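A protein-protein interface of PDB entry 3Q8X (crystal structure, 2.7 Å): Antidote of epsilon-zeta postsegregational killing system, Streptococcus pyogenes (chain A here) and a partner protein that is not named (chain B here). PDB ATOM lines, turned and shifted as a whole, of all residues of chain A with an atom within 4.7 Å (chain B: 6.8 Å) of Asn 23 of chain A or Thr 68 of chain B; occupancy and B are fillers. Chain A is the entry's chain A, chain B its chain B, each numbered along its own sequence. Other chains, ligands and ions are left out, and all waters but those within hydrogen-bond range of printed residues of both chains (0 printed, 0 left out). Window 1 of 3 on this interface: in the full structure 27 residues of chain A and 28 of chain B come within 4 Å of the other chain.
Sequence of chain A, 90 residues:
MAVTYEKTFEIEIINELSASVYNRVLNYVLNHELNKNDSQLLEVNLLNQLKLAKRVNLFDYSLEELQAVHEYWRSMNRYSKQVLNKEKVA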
ATOM      1  N   ALA A  19      25.508  -9.292 -19.396  1.00  0.00           N
ATOM      2  CA  ALA A  19      25.590  -9.472 -20.847  1.00  0.00           C
ATOM      3  C   ALA A  19      24.648  -8.499 -21.549  1.00  0.00           C
ATOM      4  O   ALA A  19      25.030  -7.873 -22.542  1.00  0.00           O
ATOM      5  CB  ALA A  19      25.297 -10.907 -21.257  1.00  0.00           C
ATOM      6  N   SER A  20      23.432  -8.359 -21.014  1.00  0.00           N
ATOM      7  CA  SER A  20      22.433  -7.433 -21.553  1.00  0.00           C
ATOM      8  C   SER A  20      22.955  -5.993 -21.638  1.00  0.00           C
ATOM      9  O   SER A  20      22.843  -5.324 -22.676  1.00  0.00           O
ATOM     10  CB  SER A  20      21.196  -7.472 -20.676  1.00  0.00           C
ATOM     11  OG  SER A  20      20.153  -6.707 -21.227  1.00  0.00           O
ATOM     12  N   VAL A  21      23.545  -5.538 -20.538  1.00  0.00           N
ATOM     13  CA  VAL A  21      24.016  -4.168 -20.405  1.00  0.00           C
ATOM     14  C   VAL A  21      25.236  -3.953 -21.284  1.00  0.00           C
ATOM     15  O   VAL A  21      25.277  -3.001 -22.050  1.00  0.00           O
ATOM     16  CB  VAL A  21      24.303  -3.796 -18.922  1.00  0.00           C
ATOM     17  CG1 VAL A  21      24.772  -2.360 -18.796  1.00  0.00           C
ATOM     18  CG2 VAL A  21      23.057  -4.012 -18.076  1.00  0.00           C
ATOM     19  N   TYR A  22      26.208  -4.850 -21.203  1.00  0.00           N
ATOM     20  CA  TYR A  22      27.377  -4.746 -22.047  1.00  0.00           C
ATOM     21  C   TYR A  22      26.963  -4.677 -23.513  1.00  0.00           C
ATOM     22  O   TYR A  22      27.421  -3.803 -24.247  1.00  0.00           O
ATOM     23  CB  TYR A  22      28.330  -5.916 -21.801  1.00  0.00           C
ATOM     24  CG  TYR A  22      29.645  -5.808 -22.540  1.00  0.00           C
ATOM     25  CD1 TYR A  22      30.647  -4.950 -22.089  1.00  0.00           C
ATOM     26  CD2 TYR A  22      29.888  -6.560 -23.693  1.00  0.00           C
ATOM     27  CE1 TYR A  22      31.862  -4.844 -22.756  1.00  0.00           C
ATOM     28  CE2 TYR A  22      31.097  -6.460 -24.375  1.00  0.00           C
ATOM     29  CZ  TYR A  22      32.092  -5.600 -23.895  1.00  0.00           C
ATOM     30  OH  TYR A  22      33.314  -5.478 -24.557  1.00  0.00           O
ATOM     31  N   ASN A  23      26.075  -5.573 -23.937  1.00  0.00           N
ATOM     32  CA  ASN A  23      25.693  -5.629 -25.341  1.00  0.00           C
ATOM     33  C   ASN A  23      24.989  -4.369 -25.845  1.00  0.00           C
ATOM     34  O   ASN A  23      25.148  -3.984 -27.002  1.00  0.00           O
ATOM     35  CB  ASN A  23      24.864  -6.874 -25.626  1.00  0.00           C
ATOM     36  CG  ASN A  23      25.724  -8.120 -25.730  1.00  0.00           C
ATOM     37  OD1 ASN A  23      26.875  -8.049 -26.170  1.00  0.00           O
ATOM     38  ND2 ASN A  23      25.184  -9.265 -25.307  1.00  0.00           N
ATOM     39  N   ARG A  24      24.219  -3.724 -24.971  1.00  0.00           N
ATOM     40  CA  ARG A  24      23.558  -2.498 -25.343  1.00  0.00           C
ATOM     41  C   ARG A  24      24.627  -1.452 -25.600  1.00  0.00           C
ATOM     42  O   ARG A  24      24.553  -0.706 -26.583  1.00  0.00           O
ATOM     43  CB  ARG A  24      22.589  -2.043 -24.251  1.00  0.00           C
ATOM     44  CG  ARG A  24      21.989  -0.646 -24.472  1.00  0.00           C
ATOM     45  CD  ARG A  24      21.114  -0.195 -23.292  1.00  0.00           C
ATOM     46  NE  ARG A  24      20.067  -1.176 -23.034  1.00  0.00           N
ATOM     47  CZ  ARG A  24      19.978  -1.924 -21.942  1.00  0.00           C
ATOM     48  NH1 ARG A  24      20.845  -1.789 -20.960  1.00  0.00           N
ATOM     49  NH2 ARG A  24      19.002  -2.804 -21.831  1.00  0.00           N
ATOM     50  N   VAL A  25      25.638  -1.414 -24.736  1.00  0.00           N
ATOM     51  CA  VAL A  25      26.688  -0.421 -24.887  1.00  0.00           C
ATOM     52  C   VAL A  25      27.570  -0.750 -26.090  1.00  0.00           C
ATOM     53  O   VAL A  25      27.890   0.140 -26.898  1.00  0.00           O
ATOM     54  CB  VAL A  25      27.510  -0.218 -23.596  1.00  0.00           C
ATOM     55  CG1 VAL A  25      28.633   0.807 -23.814  1.00  0.00           C
ATOM     56  CG2 VAL A  25      26.609   0.228 -22.471  1.00  0.00           C
ATOM     57  N   LEU A  26      27.936  -2.017 -26.237  1.00  0.00           N
ATOM     58  CA  LEU A  26      28.789  -2.406 -27.353  1.00  0.00           C
ATOM     59  C   LEU A  26      28.117  -2.075 -28.673  1.00  0.00           C
ATOM     60  O   LEU A  26      28.742  -1.471 -29.564  1.00  0.00           O
ATOM     61  CB  LEU A  26      29.141  -3.889 -27.298  1.00  0.00           C
ATOM     62  CG  LEU A  26      30.124  -4.327 -28.384  1.00  0.00           C
ATOM     63  CD1 LEU A  26      31.464  -3.562 -28.302  1.00  0.00           C
ATOM     64  CD2 LEU A  26      30.324  -5.833 -28.319  1.00  0.00           C
ATOM     65  N   ASN A  27      26.844  -2.453 -28.777  1.00  0.00           N
ATOM     66  CA  ASN A  27      26.036  -2.218 -29.978  1.00  0.00           C
ATOM     67  C   ASN A  27      26.001  -0.762 -30.403  1.00  0.00           C
ATOM     68  O   ASN A  27      26.158  -0.456 -31.566  1.00  0.00           O
ATOM     69  CB  ASN A  27      24.601  -2.731 -29.788  1.00  0.00           C
ATOM     70  CG  ASN A  27      24.354  -4.049 -30.487  1.00  0.00           C
ATOM     71  OD1 ASN A  27      25.054  -4.411 -31.431  1.00  0.00           O
ATOM     72  ND2 ASN A  27      23.342  -4.768 -30.040  1.00  0.00           N
ATOM     73  N   ASP B  18      35.501  -8.078 -30.604  1.00  0.00           N
ATOM     74  CA  ASP B  18      35.279  -7.678 -29.239  1.00  0.00           C
ATOM     75  C   ASP B  18      35.100  -8.903 -28.372  1.00  0.00           C
ATOM     76  O   ASP B  18      35.728  -9.011 -27.311  1.00  0.00           O
ATOM     77  CB  ASP B  18      34.061  -6.783 -29.114  1.00  0.00           C
ATOM     78  CG  ASP B  18      33.998  -6.109 -27.775  1.00  0.00           C
ATOM     79  OD1 ASP B  18      34.576  -5.011 -27.661  1.00  0.00           O
ATOM     80  OD2 ASP B  18      33.428  -6.699 -26.828  1.00  0.00           O
ATOM     81  N   ASN B  19      34.253  -9.823 -28.821  1.00  0.00           N
ATOM     82  CA  ASN B  19      34.040 -11.068 -28.097  1.00  0.00           C
ATOM     83  C   ASN B  19      35.350 -11.752 -27.720  1.00  0.00           C
ATOM     84  O   ASN B  19      35.521 -12.172 -26.561  1.00  0.00           O
ATOM     85  CB  ASN B  19      33.172 -12.032 -28.895  1.00  0.00           C
ATOM     86  CG  ASN B  19      31.730 -11.618 -28.931  1.00  0.00           C
ATOM     87  OD1 ASN B  19      31.208 -11.095 -27.958  1.00  0.00           O
ATOM     88  ND2 ASN B  19      31.072 -11.857 -30.058  1.00  0.00           N
ATOM     89  N   ARG B  50      30.592 -24.682 -14.227  1.00  0.00           N
ATOM     90  CA  ARG B  50      31.631 -23.684 -14.486  1.00  0.00           C
ATOM     91  C   ARG B  50      32.543 -23.524 -13.271  1.00  0.00           C
ATOM     92  O   ARG B  50      33.766 -23.411 -13.404  1.00  0.00           O
ATOM     93  CB  ARG B  50      31.024 -22.332 -14.843  1.00  0.00           C
ATOM     94  CG  ARG B  50      30.117 -22.338 -16.066  1.00  0.00           C
ATOM     95  CD  ARG B  50      29.489 -20.969 -16.242  1.00  0.00           C
ATOM     96  NE  ARG B  50      28.473 -20.911 -17.292  1.00  0.00           N
ATOM     97  CZ  ARG B  50      28.141 -19.790 -17.930  1.00  0.00           C
ATOM     98  NH1 ARG B  50      28.750 -18.645 -17.640  1.00  0.00           N
ATOM     99  NH2 ARG B  50      27.203 -19.805 -18.865  1.00  0.00           N
ATOM    100  N   VAL B  63      34.711 -19.697 -20.905  1.00  0.00           N
ATOM    101  CA  VAL B  63      33.336 -20.123 -20.964  1.00  0.00           C
ATOM    102  C   VAL B  63      32.696 -19.560 -22.216  1.00  0.00           C
ATOM    103  O   VAL B  63      32.748 -18.366 -22.458  1.00  0.00           O
ATOM    104  CB  VAL B  63      32.573 -19.656 -19.737  1.00  0.00           C
ATOM    105  CG1 VAL B  63      31.081 -19.968 -19.903  1.00  0.00           C
ATOM    106  CG2 VAL B  63      33.131 -20.340 -18.505  1.00  0.00           C
ATOM    107  N   ILE B  64      32.116 -20.437 -23.022  1.00  0.00           N
ATOM    108  CA  ILE B  64      31.451 -20.041 -24.249  1.00  0.00           C
ATOM    109  C   ILE B  64      29.966 -20.339 -24.106  1.00  0.00           C
ATOM    110  O   ILE B  64      29.554 -21.498 -23.935  1.00  0.00           O
ATOM    111  CB  ILE B  64      32.032 -20.773 -25.469  1.00  0.00           C
ATOM    112  CG1 ILE B  64      33.497 -20.368 -25.661  1.00  0.00           C
ATOM    113  CG2 ILE B  64      31.190 -20.490 -26.708  1.00  0.00           C
ATOM    114  CD1 ILE B  64      34.269 -21.251 -26.625  1.00  0.00           C
ATOM    115  N   ASP B  65      29.171 -19.277 -24.158  1.00  0.00           N
ATOM    116  CA  ASP B  65      27.752 -19.372 -23.872  1.00  0.00           C
ATOM    117  C   ASP B  65      26.905 -18.650 -24.915  1.00  0.00           C
ATOM    118  O   ASP B  65      26.847 -17.427 -24.942  1.00  0.00           O
ATOM    119  CB  ASP B  65      27.480 -18.861 -22.461  1.00  0.00           C
ATOM    120  CG  ASP B  65      26.019 -18.959 -22.081  1.00  0.00           C
ATOM    121  OD1 ASP B  65      25.280 -19.782 -22.679  1.00  0.00           O
ATOM    122  OD2 ASP B  65      25.599 -18.203 -21.179  1.00  0.00           O
ATOM    123  N   ASN B  66      26.255 -19.449 -25.762  1.00  0.00           N
ATOM    124  CA  ASN B  66      25.359 -19.018 -26.863  1.00  0.00           C
ATOM    125  C   ASN B  66      24.435 -17.871 -26.469  1.00  0.00           C
ATOM    126  O   ASN B  66      24.402 -16.850 -27.142  1.00  0.00           O
ATOM    127  CB  ASN B  66      24.554 -20.231 -27.379  1.00  0.00           C
ATOM    128  CG  ASN B  66      23.897 -19.993 -28.744  1.00  0.00           C
ATOM    129  OD1 ASN B  66      23.005 -19.139 -28.896  1.00  0.00           O
ATOM    130  ND2 ASN B  66      24.301 -20.789 -29.736  1.00  0.00           N
ATOM    131  N   ASP B  67      23.710 -18.034 -25.364  1.00  0.00           N
ATOM    132  CA  ASP B  67      22.722 -17.038 -24.924  1.00  0.00           C
ATOM    133  C   ASP B  67      23.282 -15.629 -24.697  1.00  0.00           C
ATOM    134  O   ASP B  67      22.575 -14.650 -24.884  1.00  0.00           O
ATOM    135  CB  ASP B  67      21.970 -17.507 -23.671  1.00  0.00           C
ATOM    136  CG  ASP B  67      21.128 -18.759 -23.913  1.00  0.00           C
ATOM    137  OD1 ASP B  67      20.635 -18.975 -25.058  1.00  0.00           O
ATOM    138  OD2 ASP B  67      20.949 -19.529 -22.929  1.00  0.00           O
ATOM    139  N   THR B  68      24.539 -15.514 -24.305  1.00  0.00           N
ATOM    140  CA  THR B  68      25.105 -14.189 -24.087  1.00  0.00           C
ATOM    141  C   THR B  68      25.272 -13.394 -25.384  1.00  0.00           C
ATOM    142  O   THR B  68      25.700 -12.249 -25.345  1.00  0.00           O
ATOM    143  CB  THR B  68      26.476 -14.236 -23.367  1.00  0.00           C
ATOM    144  OG1 THR B  68      27.446 -14.877 -24.206  1.00  0.00           O
ATOM    145  CG2 THR B  68      26.372 -14.966 -22.042  1.00  0.00           C
ATOM    146  N   PHE B  69      24.949 -13.997 -26.525  1.00  0.00           N
ATOM    147  CA  PHE B  69      25.172 -13.341 -27.813  1.00  0.00           C
ATOM    148  C   PHE B  69      23.900 -12.824 -28.486  1.00  0.00           C
ATOM    149  O   PHE B  69      23.962 -12.014 -29.415  1.00  0.00           O
ATOM    150  CB  PHE B  69      25.976 -14.251 -28.751  1.00  0.00           C
ATOM    151  CG  PHE B  69      27.350 -14.589 -28.225  1.00  0.00           C
ATOM    152  CD1 PHE B  69      28.266 -13.574 -27.917  1.00  0.00           C
ATOM    153  CD2 PHE B  69      27.730 -15.914 -28.029  1.00  0.00           C
ATOM    154  CE1 PHE B  69      29.536 -13.876 -27.418  1.00  0.00           C
ATOM    155  CE2 PHE B  69      28.993 -16.225 -27.522  1.00  0.00           C
ATOM    156  CZ  PHE B  69      29.896 -15.197 -27.211  1.00  0.00           C
ATOM    157  N   LYS B  70      22.755 -13.270 -27.986  1.00  0.00           N
ATOM    158  CA  LYS B  70      21.469 -12.985 -28.596  1.00  0.00           C
ATOM    159  C   LYS B  70      21.196 -11.482 -28.745  1.00  0.00           C
ATOM    160  O   LYS B  70      20.835 -11.006 -29.830  1.00  0.00           O
ATOM    161  CB  LYS B  70      20.359 -13.696 -27.813  1.00  0.00           C
ATOM    162  CG  LYS B  70      20.276 -15.195 -28.120  1.00  0.00           C
ATOM    163  CD  LYS B  70      19.364 -15.942 -27.152  1.00  0.00           C
ATOM    164  CE  LYS B  70      18.976 -17.323 -27.683  1.00  0.00           C
ATOM    165  NZ  LYS B  70      20.147 -18.217 -27.813  1.00  0.00           N
ATOM    166  N   GLN B  71      21.416 -10.742 -27.663  1.00  0.00           N
ATOM    167  CA  GLN B  71      21.175  -9.295 -27.646  1.00  0.00           C
ATOM    168  C   GLN B  71      22.271  -8.490 -28.350  1.00  0.00           C
ATOM    169  O   GLN B  71      22.181  -7.262 -28.460  1.00  0.00           O
ATOM    170  CB  GLN B  71      21.002  -8.802 -26.214  1.00  0.00           C
ATOM    171  CG  GLN B  71      19.989  -9.597 -25.395  1.00  0.00           C
ATOM    172  CD  GLN B  71      19.469  -8.819 -24.207  1.00  0.00           C
ATOM    173  OE1 GLN B  71      19.987  -7.749 -23.872  1.00  0.00           O
ATOM    174  NE2 GLN B  71      18.431  -9.339 -23.575  1.00  0.00           N
ATOM    175  N   GLN B  72      23.285  -9.197 -28.843  1.00  0.00           N
ATOM    176  CA  GLN B  72      24.428  -8.591 -29.517  1.00  0.00           C
ATOM    177  C   GLN B  72      24.164  -8.445 -31.011  1.00  0.00           C
ATOM    178  O   GLN B  72      24.970  -7.873 -31.742  1.00  0.00           O
ATOM    179  CB  GLN B  72      25.657  -9.452 -29.297  1.00  0.00           C
ATOM    180  CG  GLN B  72      26.949  -8.716 -29.301  1.00  0.00           C
ATOM    181  CD  GLN B  72      28.106  -9.672 -29.241  1.00  0.00           C
ATOM    182  OE1 GLN B  72      28.411 -10.352 -30.220  1.00  0.00           O
ATOM    183  NE2 GLN B  72      28.760  -9.737 -28.089  1.00  0.00           N
ATOM    184  N   HIS B  73      23.032  -8.969 -31.463  1.00  0.00           N
ATOM    185  CA  HIS B  73      22.594  -8.742 -32.826  1.00  0.00           C
ATOM    186  C   HIS B  73      22.633  -7.234 -33.088  1.00  0.00           C
ATOM    187  O   HIS B  73      22.218  -6.455 -32.231  1.00  0.00           O
ATOM    188  CB  HIS B  73      21.181  -9.290 -33.014  1.00  0.00           C
ATOM    189  CG  HIS B  73      20.774  -9.418 -34.446  1.00  0.00           C
ATOM    190  ND1 HIS B  73      20.441  -8.329 -35.224  1.00  0.00           N
ATOM    191  CD2 HIS B  73      20.670 -10.502 -35.249  1.00  0.00           C
ATOM    192  CE1 HIS B  73      20.148  -8.740 -36.444  1.00  0.00           C
ATOM    193  NE2 HIS B  73      20.274 -10.054 -36.484  1.00  0.00           N
ATOM    194  N   SER B  95      23.419 -15.644 -33.091  1.00  0.00           N
ATOM    195  CA  SER B  95      24.110 -16.221 -31.934  1.00  0.00           C
ATOM    196  C   SER B  95      24.758 -17.567 -32.243  1.00  0.00           C
ATOM    197  O   SER B  95      25.802 -17.897 -31.690  1.00  0.00           O
ATOM    198  CB  SER B  95      23.169 -16.354 -30.743  1.00  0.00           C
ATOM    199  OG  SER B  95      22.140 -17.274 -31.027  1.00  0.00           O
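Among the printed residues, merely in contact across the chains: Asn 23 of chain A with Gln 71 of chain B (3.9 Å) and Leu 26 of chain A with Asp 18 of chain B (3.5 Å).
Printed residues of chain A that touch a printed residue of chain B: Ser 20, Tyr 22, Asn 23, Leu 26 and Asn 27.
Hydrophobic or aromatic side chains of chain A within 4 Å of the printed part of chain B: Tyr 22 and Leu 26.
Of the 15 printed residues of chain B, 5 touch a printed residue of chain A.
Along chain B the printed residues that touch a printed residue of chain A span positions 18 to 73.
Among the printed residues, no Asp or Glu carboxylate lies within 4 Å of a Lys or Arg side-chain nitrogen of the other chain.
Of the printed residues of chain B, Tyr 22 of chain A touches Asp 18.
Of chain B, only Thr 68 (3.0 Å), Gln 71 (3.9 Å) and Gln 72 (3.2 Å) come within 4 Å of Asn 23 of chain A.
Printed residues of chain B within 4 Å of Asn 27 of chain A: Gln 71 (3.2 Å), Gln 72 (3.5 Å) and His 73 (3.0 Å).
Printed residues of chain A within 4 Å of Asp 18 of chain B: Tyr 22 and Leu 26.
Thr 68 of chain B touches one residue of chain A.
Of the printed residues of chain A, Gln 71 of chain B touches Ser 20 (2.8 Å), Asn 23 (3.9 Å) and Asn 27 (3.2 Å).
Printed residues of chain A within 4 Å of Gln 72 of chain B: Asn 23 and Asn 27.
The nearest residue of chain A that does not touch Thr 68 of chain B is Ala 19 of chain A (4.1 Å).
The nearest printed residue of chain B that does not touch Tyr 22 of chain A is Gln 72 of chain B (5.5 Å).
The side-chain amide nitrogen of Asn 23 of chain A lies within hydrogen-bond range of the backbone carbonyl oxygen of Ala 19 of chain A (3.1 Å).
The side-chain amide oxygen (OD1) of Asn 19 of chain B is in hydrogen-bond range of the side-chain amide nitrogen (NE2) of Gln 72 of chain B.
The backbone carbonyl oxygen (O) of Asp 65 of chain B sits at hydrogen-bond distance from the side-chain hydroxyl (OG1) of Thr 68 of chain B, 2.7 Å away.
The side-chain amide oxygen of Gln 71 of chain B lies within hydrogen-bond range of the side-chain hydroxyl of Ser 20 of chain A, 2.8 Å away.
The side-chain hydroxyl (OH) of Tyr 22 of chain A is in hydrogen-bond range of the side-chain carboxylate (OD2) of Asp 18 of chain B, 2.6 Å away.
The side-chain amide nitrogen of Asn 23 of chain A is in hydrogen-bond range of the backbone carbonyl oxygen of Thr 68 of chain B.
The side-chain amide oxygen of Asn 23 of chain A sits at hydrogen-bond distance from the side-chain amide nitrogen of Gln 72 of chain B, 3.2 Å away.
The backbone carbonyl oxygen (O) of Gln 71 of chain B lies within hydrogen-bond range of the side-chain amide nitrogen (ND2) of Asn 27 of chain A, at 3.2 Å.
The side-chain amide oxygen (OD1) of Asn 27 of chain A lies close to the backbone carbonyl oxygen (O) of Gln 72 of chain B, at 3.5 Å.
The backbone carbonyl oxygen (O) of His 73 of chain B sits at hydrogen-bond distance from the side-chain amide nitrogen (ND2) of Asn 27 of chain A.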
